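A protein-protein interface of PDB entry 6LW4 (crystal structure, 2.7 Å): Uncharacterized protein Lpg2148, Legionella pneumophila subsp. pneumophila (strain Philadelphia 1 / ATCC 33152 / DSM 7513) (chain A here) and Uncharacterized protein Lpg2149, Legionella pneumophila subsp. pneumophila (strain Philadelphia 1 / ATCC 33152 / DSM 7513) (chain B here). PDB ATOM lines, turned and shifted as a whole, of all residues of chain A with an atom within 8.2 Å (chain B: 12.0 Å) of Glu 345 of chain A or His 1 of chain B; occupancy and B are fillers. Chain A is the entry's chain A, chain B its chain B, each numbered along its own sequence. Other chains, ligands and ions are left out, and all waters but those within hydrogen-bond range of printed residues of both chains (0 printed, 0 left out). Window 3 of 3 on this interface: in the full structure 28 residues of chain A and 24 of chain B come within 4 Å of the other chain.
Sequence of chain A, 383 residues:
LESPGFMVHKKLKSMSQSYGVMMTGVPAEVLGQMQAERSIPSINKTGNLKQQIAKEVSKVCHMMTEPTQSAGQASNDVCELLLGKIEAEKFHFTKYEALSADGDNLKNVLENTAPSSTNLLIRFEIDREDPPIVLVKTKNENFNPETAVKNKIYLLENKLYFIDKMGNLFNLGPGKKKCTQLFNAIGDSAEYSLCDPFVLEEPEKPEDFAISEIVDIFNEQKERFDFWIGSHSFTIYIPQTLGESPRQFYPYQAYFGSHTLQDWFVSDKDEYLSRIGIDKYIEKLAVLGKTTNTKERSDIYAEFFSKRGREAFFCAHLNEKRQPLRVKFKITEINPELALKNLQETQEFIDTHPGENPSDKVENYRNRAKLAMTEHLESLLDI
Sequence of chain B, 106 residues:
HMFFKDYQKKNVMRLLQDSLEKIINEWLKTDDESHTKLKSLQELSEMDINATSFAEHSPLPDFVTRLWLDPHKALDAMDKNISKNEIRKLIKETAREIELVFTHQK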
ATOM      1  N   LYS A  11      -0.665  22.441 -22.200  1.00  0.00           N
ATOM      2  CA  LYS A  11      -1.478  21.236 -22.099  1.00  0.00           C
ATOM      3  C   LYS A  11      -1.239  20.516 -20.778  1.00  0.00           C
ATOM      4  O   LYS A  11      -2.184  20.004 -20.173  1.00  0.00           O
ATOM      5  CB  LYS A  11      -1.205  20.306 -23.282  1.00  0.00           C
ATOM      6  CG  LYS A  11      -2.444  19.544 -23.753  1.00  0.00           C
ATOM      7  CD  LYS A  11      -2.105  18.165 -24.306  1.00  0.00           C
ATOM      8  CE  LYS A  11      -2.975  17.805 -25.508  1.00  0.00           C
ATOM      9  NZ  LYS A  11      -4.406  17.605 -25.132  1.00  0.00           N
ATOM     10  N   MET A  15      -4.262  20.107 -18.197  1.00  0.00           N
ATOM     11  CA  MET A  15      -4.738  18.750 -17.969  1.00  0.00           C
ATOM     12  C   MET A  15      -4.607  18.356 -16.505  1.00  0.00           C
ATOM     13  O   MET A  15      -5.454  17.625 -15.978  1.00  0.00           O
ATOM     14  CB  MET A  15      -3.966  17.773 -18.848  1.00  0.00           C
ATOM     15  CG  MET A  15      -4.508  17.632 -20.255  1.00  0.00           C
ATOM     16  SD  MET A  15      -3.452  16.597 -21.300  1.00  0.00           S
ATOM     17  CE  MET A  15      -3.765  14.965 -20.642  1.00  0.00           C
ATOM     18  N   LEU A  81       6.424  12.111 -18.766  1.00  0.00           N
ATOM     19  CA  LEU A  81       5.511  12.728 -19.722  1.00  0.00           C
ATOM     20  C   LEU A  81       6.266  13.523 -20.781  1.00  0.00           C
ATOM     21  O   LEU A  81       5.920  13.469 -21.969  1.00  0.00           O
ATOM     22  CB  LEU A  81       4.519  13.634 -18.992  1.00  0.00           C
ATOM     23  CG  LEU A  81       3.383  12.966 -18.220  1.00  0.00           C
ATOM     24  CD1 LEU A  81       2.728  13.962 -17.279  1.00  0.00           C
ATOM     25  CD2 LEU A  81       2.356  12.371 -19.169  1.00  0.00           C
ATOM     26  N   LEU A 338       7.117  14.707 -29.146  1.00  0.00           N
ATOM     27  CA  LEU A 338       6.959  13.485 -28.366  1.00  0.00           C
ATOM     28  C   LEU A 338       6.221  13.755 -27.059  1.00  0.00           C
ATOM     29  O   LEU A 338       5.392  12.942 -26.629  1.00  0.00           O
ATOM     30  CB  LEU A 338       8.321  12.852 -28.092  1.00  0.00           C
ATOM     31  CG  LEU A 338       8.279  11.534 -27.317  1.00  0.00           C
ATOM     32  CD1 LEU A 338       7.693  10.421 -28.177  1.00  0.00           C
ATOM     33  CD2 LEU A 338       9.666  11.160 -26.835  1.00  0.00           C
ATOM     34  N   ALA A 339       6.507  14.891 -26.415  1.00  0.00           N
ATOM     35  CA  ALA A 339       5.781  15.245 -25.199  1.00  0.00           C
ATOM     36  C   ALA A 339       4.295  15.429 -25.481  1.00  0.00           C
ATOM     37  O   ALA A 339       3.447  14.979 -24.700  1.00  0.00           O
ATOM     38  CB  ALA A 339       6.374  16.512 -24.584  1.00  0.00           C
ATOM     39  N   LEU A 340       3.960  16.077 -26.600  1.00  0.00           N
ATOM     40  CA  LEU A 340       2.557  16.260 -26.952  1.00  0.00           C
ATOM     41  C   LEU A 340       1.886  14.930 -27.288  1.00  0.00           C
ATOM     42  O   LEU A 340       0.709  14.731 -26.976  1.00  0.00           O
ATOM     43  CB  LEU A 340       2.433  17.241 -28.117  1.00  0.00           C
ATOM     44  CG  LEU A 340       2.715  18.711 -27.793  1.00  0.00           C
ATOM     45  CD1 LEU A 340       2.596  19.562 -29.042  1.00  0.00           C
ATOM     46  CD2 LEU A 340       1.786  19.230 -26.707  1.00  0.00           C
ATOM     47  N   LYS A 341       2.620  13.996 -27.901  1.00  0.00           N
ATOM     48  CA  LYS A 341       2.033  12.683 -28.170  1.00  0.00           C
ATOM     49  C   LYS A 341       1.799  11.903 -26.878  1.00  0.00           C
ATOM     50  O   LYS A 341       0.791  11.190 -26.743  1.00  0.00           O
ATOM     51  CB  LYS A 341       2.921  11.893 -29.132  1.00  0.00           C
ATOM     52  CG  LYS A 341       2.960  12.481 -30.539  1.00  0.00           C
ATOM     53  CD  LYS A 341       3.353  11.453 -31.589  1.00  0.00           C
ATOM     54  CE  LYS A 341       4.280  12.068 -32.632  1.00  0.00           C
ATOM     55  NZ  LYS A 341       4.244  11.334 -33.929  1.00  0.00           N
ATOM     56  N   ASN A 342       2.715  12.030 -25.915  1.00  0.00           N
ATOM     57  CA  ASN A 342       2.507  11.428 -24.600  1.00  0.00           C
ATOM     58  C   ASN A 342       1.261  11.997 -23.935  1.00  0.00           C
ATOM     59  O   ASN A 342       0.421  11.253 -23.404  1.00  0.00           O
ATOM     60  CB  ASN A 342       3.735  11.664 -23.721  1.00  0.00           C
ATOM     61  CG  ASN A 342       4.967  10.967 -24.242  1.00  0.00           C
ATOM     62  OD1 ASN A 342       4.891  10.141 -25.154  1.00  0.00           O
ATOM     63  ND2 ASN A 342       6.117  11.306 -23.676  1.00  0.00           N
ATOM     64  N   LEU A 343       1.133  13.325 -23.951  1.00  0.00           N
ATOM     65  CA  LEU A 343      -0.052  13.959 -23.387  1.00  0.00           C
ATOM     66  C   LEU A 343      -1.316  13.543 -24.129  1.00  0.00           C
ATOM     67  O   LEU A 343      -2.381  13.422 -23.516  1.00  0.00           O
ATOM     68  CB  LEU A 343       0.118  15.476 -23.404  1.00  0.00           C
ATOM     69  CG  LEU A 343       1.245  15.974 -22.498  1.00  0.00           C
ATOM     70  CD1 LEU A 343       1.584  17.428 -22.778  1.00  0.00           C
ATOM     71  CD2 LEU A 343       0.866  15.779 -21.037  1.00  0.00           C
ATOM     72  N   GLN A 344      -1.216  13.294 -25.436  1.00  0.00           N
ATOM     73  CA  GLN A 344      -2.378  12.854 -26.200  1.00  0.00           C
ATOM     74  C   GLN A 344      -2.802  11.441 -25.807  1.00  0.00           C
ATOM     75  O   GLN A 344      -4.000  11.155 -25.697  1.00  0.00           O
ATOM     76  CB  GLN A 344      -2.075  12.937 -27.698  1.00  0.00           C
ATOM     77  CG  GLN A 344      -3.276  12.708 -28.599  1.00  0.00           C
ATOM     78  CD  GLN A 344      -4.465  13.565 -28.207  1.00  0.00           C
ATOM     79  OE1 GLN A 344      -4.357  14.787 -28.099  1.00  0.00           O
ATOM     80  NE2 GLN A 344      -5.610  12.924 -27.982  1.00  0.00           N
ATOM     81  N   GLU A 345      -1.839  10.542 -25.592  1.00  0.00           N
ATOM     82  CA  GLU A 345      -2.198   9.204 -25.124  1.00  0.00           C
ATOM     83  C   GLU A 345      -2.815   9.260 -23.729  1.00  0.00           C
ATOM     84  O   GLU A 345      -3.773   8.529 -23.428  1.00  0.00           O
ATOM     85  CB  GLU A 345      -0.975   8.287 -25.146  1.00  0.00           C
ATOM     86  CG  GLU A 345      -0.825   7.508 -26.439  1.00  0.00           C
ATOM     87  CD  GLU A 345       0.072   6.296 -26.294  1.00  0.00           C
ATOM     88  OE1 GLU A 345       1.311   6.464 -26.332  1.00  0.00           O
ATOM     89  OE2 GLU A 345      -0.460   5.174 -26.149  1.00  0.00           O
ATOM     90  N   THR A 346      -2.291  10.139 -22.866  1.00  0.00           N
ATOM     91  CA  THR A 346      -2.894  10.319 -21.547  1.00  0.00           C
ATOM     92  C   THR A 346      -4.321  10.850 -21.662  1.00  0.00           C
ATOM     93  O   THR A 346      -5.224  10.398 -20.945  1.00  0.00           O
ATOM     94  CB  THR A 346      -2.038  11.261 -20.699  1.00  0.00           C
ATOM     95  OG1 THR A 346      -0.655  10.907 -20.831  1.00  0.00           O
ATOM     96  CG2 THR A 346      -2.439  11.169 -19.236  1.00  0.00           C
ATOM     97  N   GLN A 347      -4.539  11.809 -22.567  1.00  0.00           N
ATOM     98  CA  GLN A 347      -5.874  12.350 -22.791  1.00  0.00           C
ATOM     99  C   GLN A 347      -6.821  11.297 -23.347  1.00  0.00           C
ATOM    100  O   GLN A 347      -8.016  11.327 -23.050  1.00  0.00           O
ATOM    101  CB  GLN A 347      -5.799  13.547 -23.738  1.00  0.00           C
ATOM    102  CG  GLN A 347      -7.133  14.231 -23.995  1.00  0.00           C
ATOM    103  CD  GLN A 347      -7.720  14.865 -22.750  1.00  0.00           C
ATOM    104  OE1 GLN A 347      -7.286  15.934 -22.321  1.00  0.00           O
ATOM    105  NE2 GLN A 347      -8.715  14.210 -22.164  1.00  0.00           N
ATOM    106  N   GLU A 348      -6.312  10.365 -24.156  1.00  0.00           N
ATOM    107  CA  GLU A 348      -7.143   9.253 -24.611  1.00  0.00           C
ATOM    108  C   GLU A 348      -7.570   8.384 -23.435  1.00  0.00           C
ATOM    109  O   GLU A 348      -8.750   8.019 -23.308  1.00  0.00           O
ATOM    110  CB  GLU A 348      -6.391   8.420 -25.653  1.00  0.00           C
ATOM    111  CG  GLU A 348      -6.267   9.079 -27.022  1.00  0.00           C
ATOM    112  CD  GLU A 348      -5.365   8.305 -27.975  1.00  0.00           C
ATOM    113  OE1 GLU A 348      -5.052   7.130 -27.687  1.00  0.00           O
ATOM    114  OE2 GLU A 348      -4.953   8.883 -29.006  1.00  0.00           O
ATOM    115  N   PHE A 349      -6.618   8.044 -22.559  1.00  0.00           N
ATOM    116  CA  PHE A 349      -6.963   7.316 -21.339  1.00  0.00           C
ATOM    117  C   PHE A 349      -8.062   8.038 -20.567  1.00  0.00           C
ATOM    118  O   PHE A 349      -9.046   7.427 -20.134  1.00  0.00           O
ATOM    119  CB  PHE A 349      -5.727   7.134 -20.457  1.00  0.00           C
ATOM    120  CG  PHE A 349      -6.046   6.764 -19.025  1.00  0.00           C
ATOM    121  CD1 PHE A 349      -6.421   5.470 -18.694  1.00  0.00           C
ATOM    122  CD2 PHE A 349      -5.957   7.710 -18.008  1.00  0.00           C
ATOM    123  CE1 PHE A 349      -6.710   5.126 -17.386  1.00  0.00           C
ATOM    124  CE2 PHE A 349      -6.247   7.372 -16.694  1.00  0.00           C
ATOM    125  CZ  PHE A 349      -6.624   6.077 -16.384  1.00  0.00           C
ATOM    126  N   ILE A 350      -7.908   9.350 -20.395  1.00  0.00           N
ATOM    127  CA  ILE A 350      -8.918  10.127 -19.678  1.00  0.00           C
ATOM    128  C   ILE A 350     -10.259  10.052 -20.402  1.00  0.00           C
ATOM    129  O   ILE A 350     -11.306   9.810 -19.786  1.00  0.00           O
ATOM    130  CB  ILE A 350      -8.446  11.580 -19.500  1.00  0.00           C
ATOM    131  CG1 ILE A 350      -7.395  11.649 -18.393  1.00  0.00           C
ATOM    132  CG2 ILE A 350      -9.621  12.483 -19.177  1.00  0.00           C
ATOM    133  CD1 ILE A 350      -6.610  12.931 -18.380  1.00  0.00           C
ATOM    134  N   ASP A 351     -10.243  10.236 -21.725  1.00  0.00           N
ATOM    135  CA  ASP A 351     -11.464  10.220 -22.520  1.00  0.00           C
ATOM    136  C   ASP A 351     -12.161   8.869 -22.491  1.00  0.00           C
ATOM    137  O   ASP A 351     -13.342   8.792 -22.847  1.00  0.00           O
ATOM    138  CB  ASP A 351     -11.157  10.612 -23.967  1.00  0.00           C
ATOM    139  CG  ASP A 351     -10.963  12.104 -24.136  1.00  0.00           C
ATOM    140  OD1 ASP A 351     -11.248  12.852 -23.177  1.00  0.00           O
ATOM    141  OD2 ASP A 351     -10.529  12.531 -25.227  1.00  0.00           O
ATOM    142  N   THR A 352     -11.468   7.800 -22.084  1.00  0.00           N
ATOM    143  CA  THR A 352     -12.191   6.552 -21.842  1.00  0.00           C
ATOM    144  C   THR A 352     -13.169   6.657 -20.673  1.00  0.00           C
ATOM    145  O   THR A 352     -13.946   5.722 -20.455  1.00  0.00           O
ATOM    146  CB  THR A 352     -11.223   5.387 -21.591  1.00  0.00           C
ATOM    147  OG1 THR A 352     -10.464   5.627 -20.400  1.00  0.00           O
ATOM    148  CG2 THR A 352     -10.271   5.213 -22.763  1.00  0.00           C
ATOM    149  N   HIS B   1       2.640   4.363 -30.417  1.00  0.00           N
ATOM    150  CA  HIS B   1       2.005   4.504 -29.112  1.00  0.00           C
ATOM    151  C   HIS B   1       2.982   4.139 -27.999  1.00  0.00           C
ATOM    152  O   HIS B   1       3.954   4.860 -27.755  1.00  0.00           O
ATOM    153  CB  HIS B   1       0.755   3.635 -29.030  1.00  0.00           C
ATOM    154  N   MET B   2       2.681   3.031 -27.313  1.00  0.00           N
ATOM    155  CA  MET B   2       3.571   2.373 -26.357  1.00  0.00           C
ATOM    156  C   MET B   2       3.801   3.165 -25.072  1.00  0.00           C
ATOM    157  O   MET B   2       4.054   2.569 -24.018  1.00  0.00           O
ATOM    158  CB  MET B   2       4.918   2.056 -27.017  1.00  0.00           C
ATOM    159  N   PHE B   3       3.713   4.497 -25.135  1.00  0.00           N
ATOM    160  CA  PHE B   3       4.133   5.319 -24.003  1.00  0.00           C
ATOM    161  C   PHE B   3       3.259   5.081 -22.778  1.00  0.00           C
ATOM    162  O   PHE B   3       3.768   4.801 -21.685  1.00  0.00           O
ATOM    163  CB  PHE B   3       4.111   6.802 -24.377  1.00  0.00           C
ATOM    164  CG  PHE B   3       4.044   7.717 -23.183  1.00  0.00           C
ATOM    165  CD1 PHE B   3       5.186   8.008 -22.455  1.00  0.00           C
ATOM    166  CD2 PHE B   3       2.837   8.267 -22.773  1.00  0.00           C
ATOM    167  CE1 PHE B   3       5.128   8.839 -21.347  1.00  0.00           C
ATOM    168  CE2 PHE B   3       2.771   9.093 -21.663  1.00  0.00           C
ATOM    169  CZ  PHE B   3       3.919   9.381 -20.951  1.00  0.00           C
ATOM    170  N   PHE B   4       1.937   5.195 -22.937  1.00  0.00           N
ATOM    171  CA  PHE B   4       1.073   5.319 -21.767  1.00  0.00           C
ATOM    172  C   PHE B   4       1.025   4.037 -20.945  1.00  0.00           C
ATOM    173  O   PHE B   4       0.900   4.095 -19.719  1.00  0.00           O
ATOM    174  CB  PHE B   4      -0.343   5.718 -22.173  1.00  0.00           C
ATOM    175  CG  PHE B   4      -1.273   5.833 -21.004  1.00  0.00           C
ATOM    176  CD1 PHE B   4      -1.324   7.003 -20.262  1.00  0.00           C
ATOM    177  CD2 PHE B   4      -2.064   4.760 -20.619  1.00  0.00           C
ATOM    178  CE1 PHE B   4      -2.162   7.108 -19.166  1.00  0.00           C
ATOM    179  CE2 PHE B   4      -2.901   4.859 -19.524  1.00  0.00           C
ATOM    180  CZ  PHE B   4      -2.946   6.033 -18.795  1.00  0.00           C
ATOM    181  N   LYS B   5       1.083   2.873 -21.591  1.00  0.00           N
ATOM    182  CA  LYS B   5       0.936   1.627 -20.844  1.00  0.00           C
ATOM    183  C   LYS B   5       2.037   1.471 -19.800  1.00  0.00           C
ATOM    184  O   LYS B   5       1.760   1.122 -18.646  1.00  0.00           O
ATOM    185  CB  LYS B   5       0.917   0.433 -21.800  1.00  0.00           C
ATOM    186  CG  LYS B   5      -0.476   0.054 -22.275  1.00  0.00           C
ATOM    187  CD  LYS B   5      -1.381  -0.262 -21.093  1.00  0.00           C
ATOM    188  CE  LYS B   5      -2.839  -0.392 -21.510  1.00  0.00           C
ATOM    189  NZ  LYS B   5      -3.136  -1.729 -22.089  1.00  0.00           N
ATOM    190  N   ASP B   6       3.287   1.753 -20.170  1.00  0.00           N
ATOM    191  CA  ASP B   6       4.379   1.597 -19.211  1.00  0.00           C
ATOM    192  C   ASP B   6       4.403   2.720 -18.180  1.00  0.00           C
ATOM    193  O   ASP B   6       4.833   2.504 -17.043  1.00  0.00           O
ATOM    194  CB  ASP B   6       5.719   1.513 -19.946  1.00  0.00           C
ATOM    195  CG  ASP B   6       6.071   0.092 -20.342  1.00  0.00           C
ATOM    196  OD1 ASP B   6       5.648  -0.347 -21.434  1.00  0.00           O
ATOM    197  OD2 ASP B   6       6.764  -0.588 -19.553  1.00  0.00           O
ATOM    198  N   TYR B   7       3.942   3.912 -18.553  1.00  0.00           N
ATOM    199  CA  TYR B   7       3.781   4.995 -17.588  1.00  0.00           C
ATOM    200  C   TYR B   7       2.756   4.616 -16.520  1.00  0.00           C
ATOM    201  O   TYR B   7       2.991   4.772 -15.310  1.00  0.00           O
ATOM    202  CB  TYR B   7       3.370   6.254 -18.351  1.00  0.00           C
ATOM    203  CG  TYR B   7       2.914   7.434 -17.531  1.00  0.00           C
ATOM    204  CD1 TYR B   7       3.832   8.280 -16.923  1.00  0.00           C
ATOM    205  CD2 TYR B   7       1.565   7.729 -17.404  1.00  0.00           C
ATOM    206  CE1 TYR B   7       3.415   9.373 -16.192  1.00  0.00           C
ATOM    207  CE2 TYR B   7       1.140   8.818 -16.677  1.00  0.00           C
ATOM    208  CZ  TYR B   7       2.067   9.636 -16.072  1.00  0.00           C
ATOM    209  OH  TYR B   7       1.644  10.722 -15.343  1.00  0.00           O
ATOM    210  N   GLN B   8       1.615   4.088 -16.960  1.00  0.00           N
ATOM    211  CA  GLN B   8       0.615   3.573 -16.036  1.00  0.00           C
ATOM    212  C   GLN B   8       1.180   2.443 -15.187  1.00  0.00           C
ATOM    213  O   GLN B   8       0.920   2.378 -13.982  1.00  0.00           O
ATOM    214  CB  GLN B   8      -0.613   3.106 -16.820  1.00  0.00           C
ATOM    215  CG  GLN B   8      -1.625   2.324 -16.007  1.00  0.00           C
ATOM    216  CD  GLN B   8      -2.844   1.943 -16.820  1.00  0.00           C
ATOM    217  OE1 GLN B   8      -2.876   0.893 -17.466  1.00  0.00           O
ATOM    218  NE2 GLN B   8      -3.860   2.799 -16.794  1.00  0.00           N
ATOM    219  N   LYS B   9       1.954   1.541 -15.798  1.00  0.00           N
ATOM    220  CA  LYS B   9       2.517   0.416 -15.057  1.00  0.00           C
ATOM    221  C   LYS B   9       3.442   0.898 -13.947  1.00  0.00           C
ATOM    222  O   LYS B   9       3.356   0.432 -12.805  1.00  0.00           O
ATOM    223  CB  LYS B   9       3.264  -0.524 -16.005  1.00  0.00           C
ATOM    224  CG  LYS B   9       4.111  -1.578 -15.298  1.00  0.00           C
ATOM    225  CD  LYS B   9       4.828  -2.479 -16.294  1.00  0.00           C
ATOM    226  CE  LYS B   9       5.476  -3.672 -15.602  1.00  0.00           C
ATOM    227  NZ  LYS B   9       5.741  -4.793 -16.550  1.00  0.00           N
ATOM    228  N   ASN B  11       3.503   3.816 -12.475  1.00  0.00           N
ATOM    229  CA  ASN B  11       2.767   4.504 -11.418  1.00  0.00           C
ATOM    230  C   ASN B  11       1.972   3.525 -10.556  1.00  0.00           C
ATOM    231  O   ASN B  11       1.889   3.696  -9.332  1.00  0.00           O
ATOM    232  CB  ASN B  11       1.863   5.577 -12.015  1.00  0.00           C
ATOM    233  CG  ASN B  11       2.589   6.890 -12.222  1.00  0.00           C
ATOM    234  OD1 ASN B  11       3.676   7.094 -11.683  1.00  0.00           O
ATOM    235  ND2 ASN B  11       1.994   7.790 -12.997  1.00  0.00           N
ATOM    236  N   ASP B  79      -3.370  -4.600 -13.986  1.00  0.00           N
ATOM    237  CA  ASP B  79      -3.165  -5.085 -15.343  1.00  0.00           C
ATOM    238  C   ASP B  79      -2.203  -6.266 -15.351  1.00  0.00           C
ATOM    239  O   ASP B  79      -1.313  -6.382 -14.501  1.00  0.00           O
ATOM    240  CB  ASP B  79      -2.625  -3.975 -16.245  1.00  0.00           C
ATOM    241  CG  ASP B  79      -2.857  -4.260 -17.720  1.00  0.00           C
ATOM    242  OD1 ASP B  79      -3.112  -5.435 -18.066  1.00  0.00           O
ATOM    243  OD2 ASP B  79      -2.772  -3.314 -18.535  1.00  0.00           O
ATOM    244  N   ASN B  81       0.017  -6.769 -17.564  1.00  0.00           N
ATOM    245  CA  ASN B  81       1.348  -6.387 -18.021  1.00  0.00           C
ATOM    246  C   ASN B  81       2.333  -6.273 -16.868  1.00  0.00           C
ATOM    247  O   ASN B  81       3.515  -5.991 -17.096  1.00  0.00           O
ATOM    248  CB  ASN B  81       1.300  -5.068 -18.803  1.00  0.00           C
ATOM    249  CG  ASN B  81       0.693  -3.924 -18.008  1.00  0.00           C
ATOM    250  OD1 ASN B  81       0.569  -3.991 -16.786  1.00  0.00           O
ATOM    251  ND2 ASN B  81       0.322  -2.858 -18.707  1.00  0.00           N
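Of the 18 printed residues of chain A, 5 touch a printed residue of chain B. Printed residues of chain B that touch a printed residue of chain A: His 1, Met 2, Phe 3, Phe 4, Tyr 7 and Gln 8. Hydrophobic or aromatic side chains of chain B that line the printed part of chain A: His 1, Phe 3, Phe 4 and Tyr 7.
Leu 338 of chain A touches none of the printed residues of chain B. No residue of chain B comes within 4 Å of Gln 344 of chain A. Of the printed residues of chain B, Thr 346 of chain A touches Phe 3 and Phe 4. No residue of chain B comes within 4 Å of Glu 348 of chain A. Printed residues of chain B within 4 Å of Phe 349 of chain A: Phe 4 and Gln 8. Of the printed residues of chain A, His 1 of chain B touches Glu 345 (3.3 Å). Asp 6 of chain B touches none of the printed residues of chain A. Printed residues of chain A within 4 Å of Tyr 7 of chain B: Leu 81. The nearest residue of chain B that does not touch Glu 345 of chain A is Lys 5 of chain B (5.3 Å). The nearest printed residue of chain A that does not touch Phe 4 of chain B is Asn 342 of chain A (5.6 Å).
The side-chain carboxylate (OE1) of Glu 345 of chain A sits at hydrogen-bond distance from the backbone NH (N) of Phe 3 of chain B. OE1 of Glu 345 of chain A sits close to O of His 1 of chain B (3.4 Å).
O of Leu 338 of chain A sits close to OD1 of Asn 342 of chain A, at 3.2 Å. The backbone carbonyl oxygen (O) of Asn 342 of chain A lies within hydrogen-bond range of the side-chain hydroxyl (OG1) of Thr 346 of chain A, 2.8 Å away. O of Leu 81 of chain A is in hydrogen-bond range of ND2 of Asn 342 of chain A (2.8 Å).
Among the printed residues, merely in contact across the chains: Phe 349 of chain A with Phe 4 of chain B (3.2 Å), Asn 342 of chain A with Phe 3 of chain B (3.2 Å), Glu 345 of chain A with Phe 4 of chain B (3.7 Å), Phe 349 of chain A with Gln 8 of chain B (3.7 Å), Leu 81 of chain A with Phe 3 of chain B (3.8 Å), Glu 345 of chain A with Met 2 of chain B (3.8 Å), Thr 346 of chain A with Phe 4 of chain B (3.9 Å), Leu 81 of chain A with Tyr 7 of chain B (3.9 Å) and Thr 346 of chain A with Phe 3 of chain B (3.96 Å).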
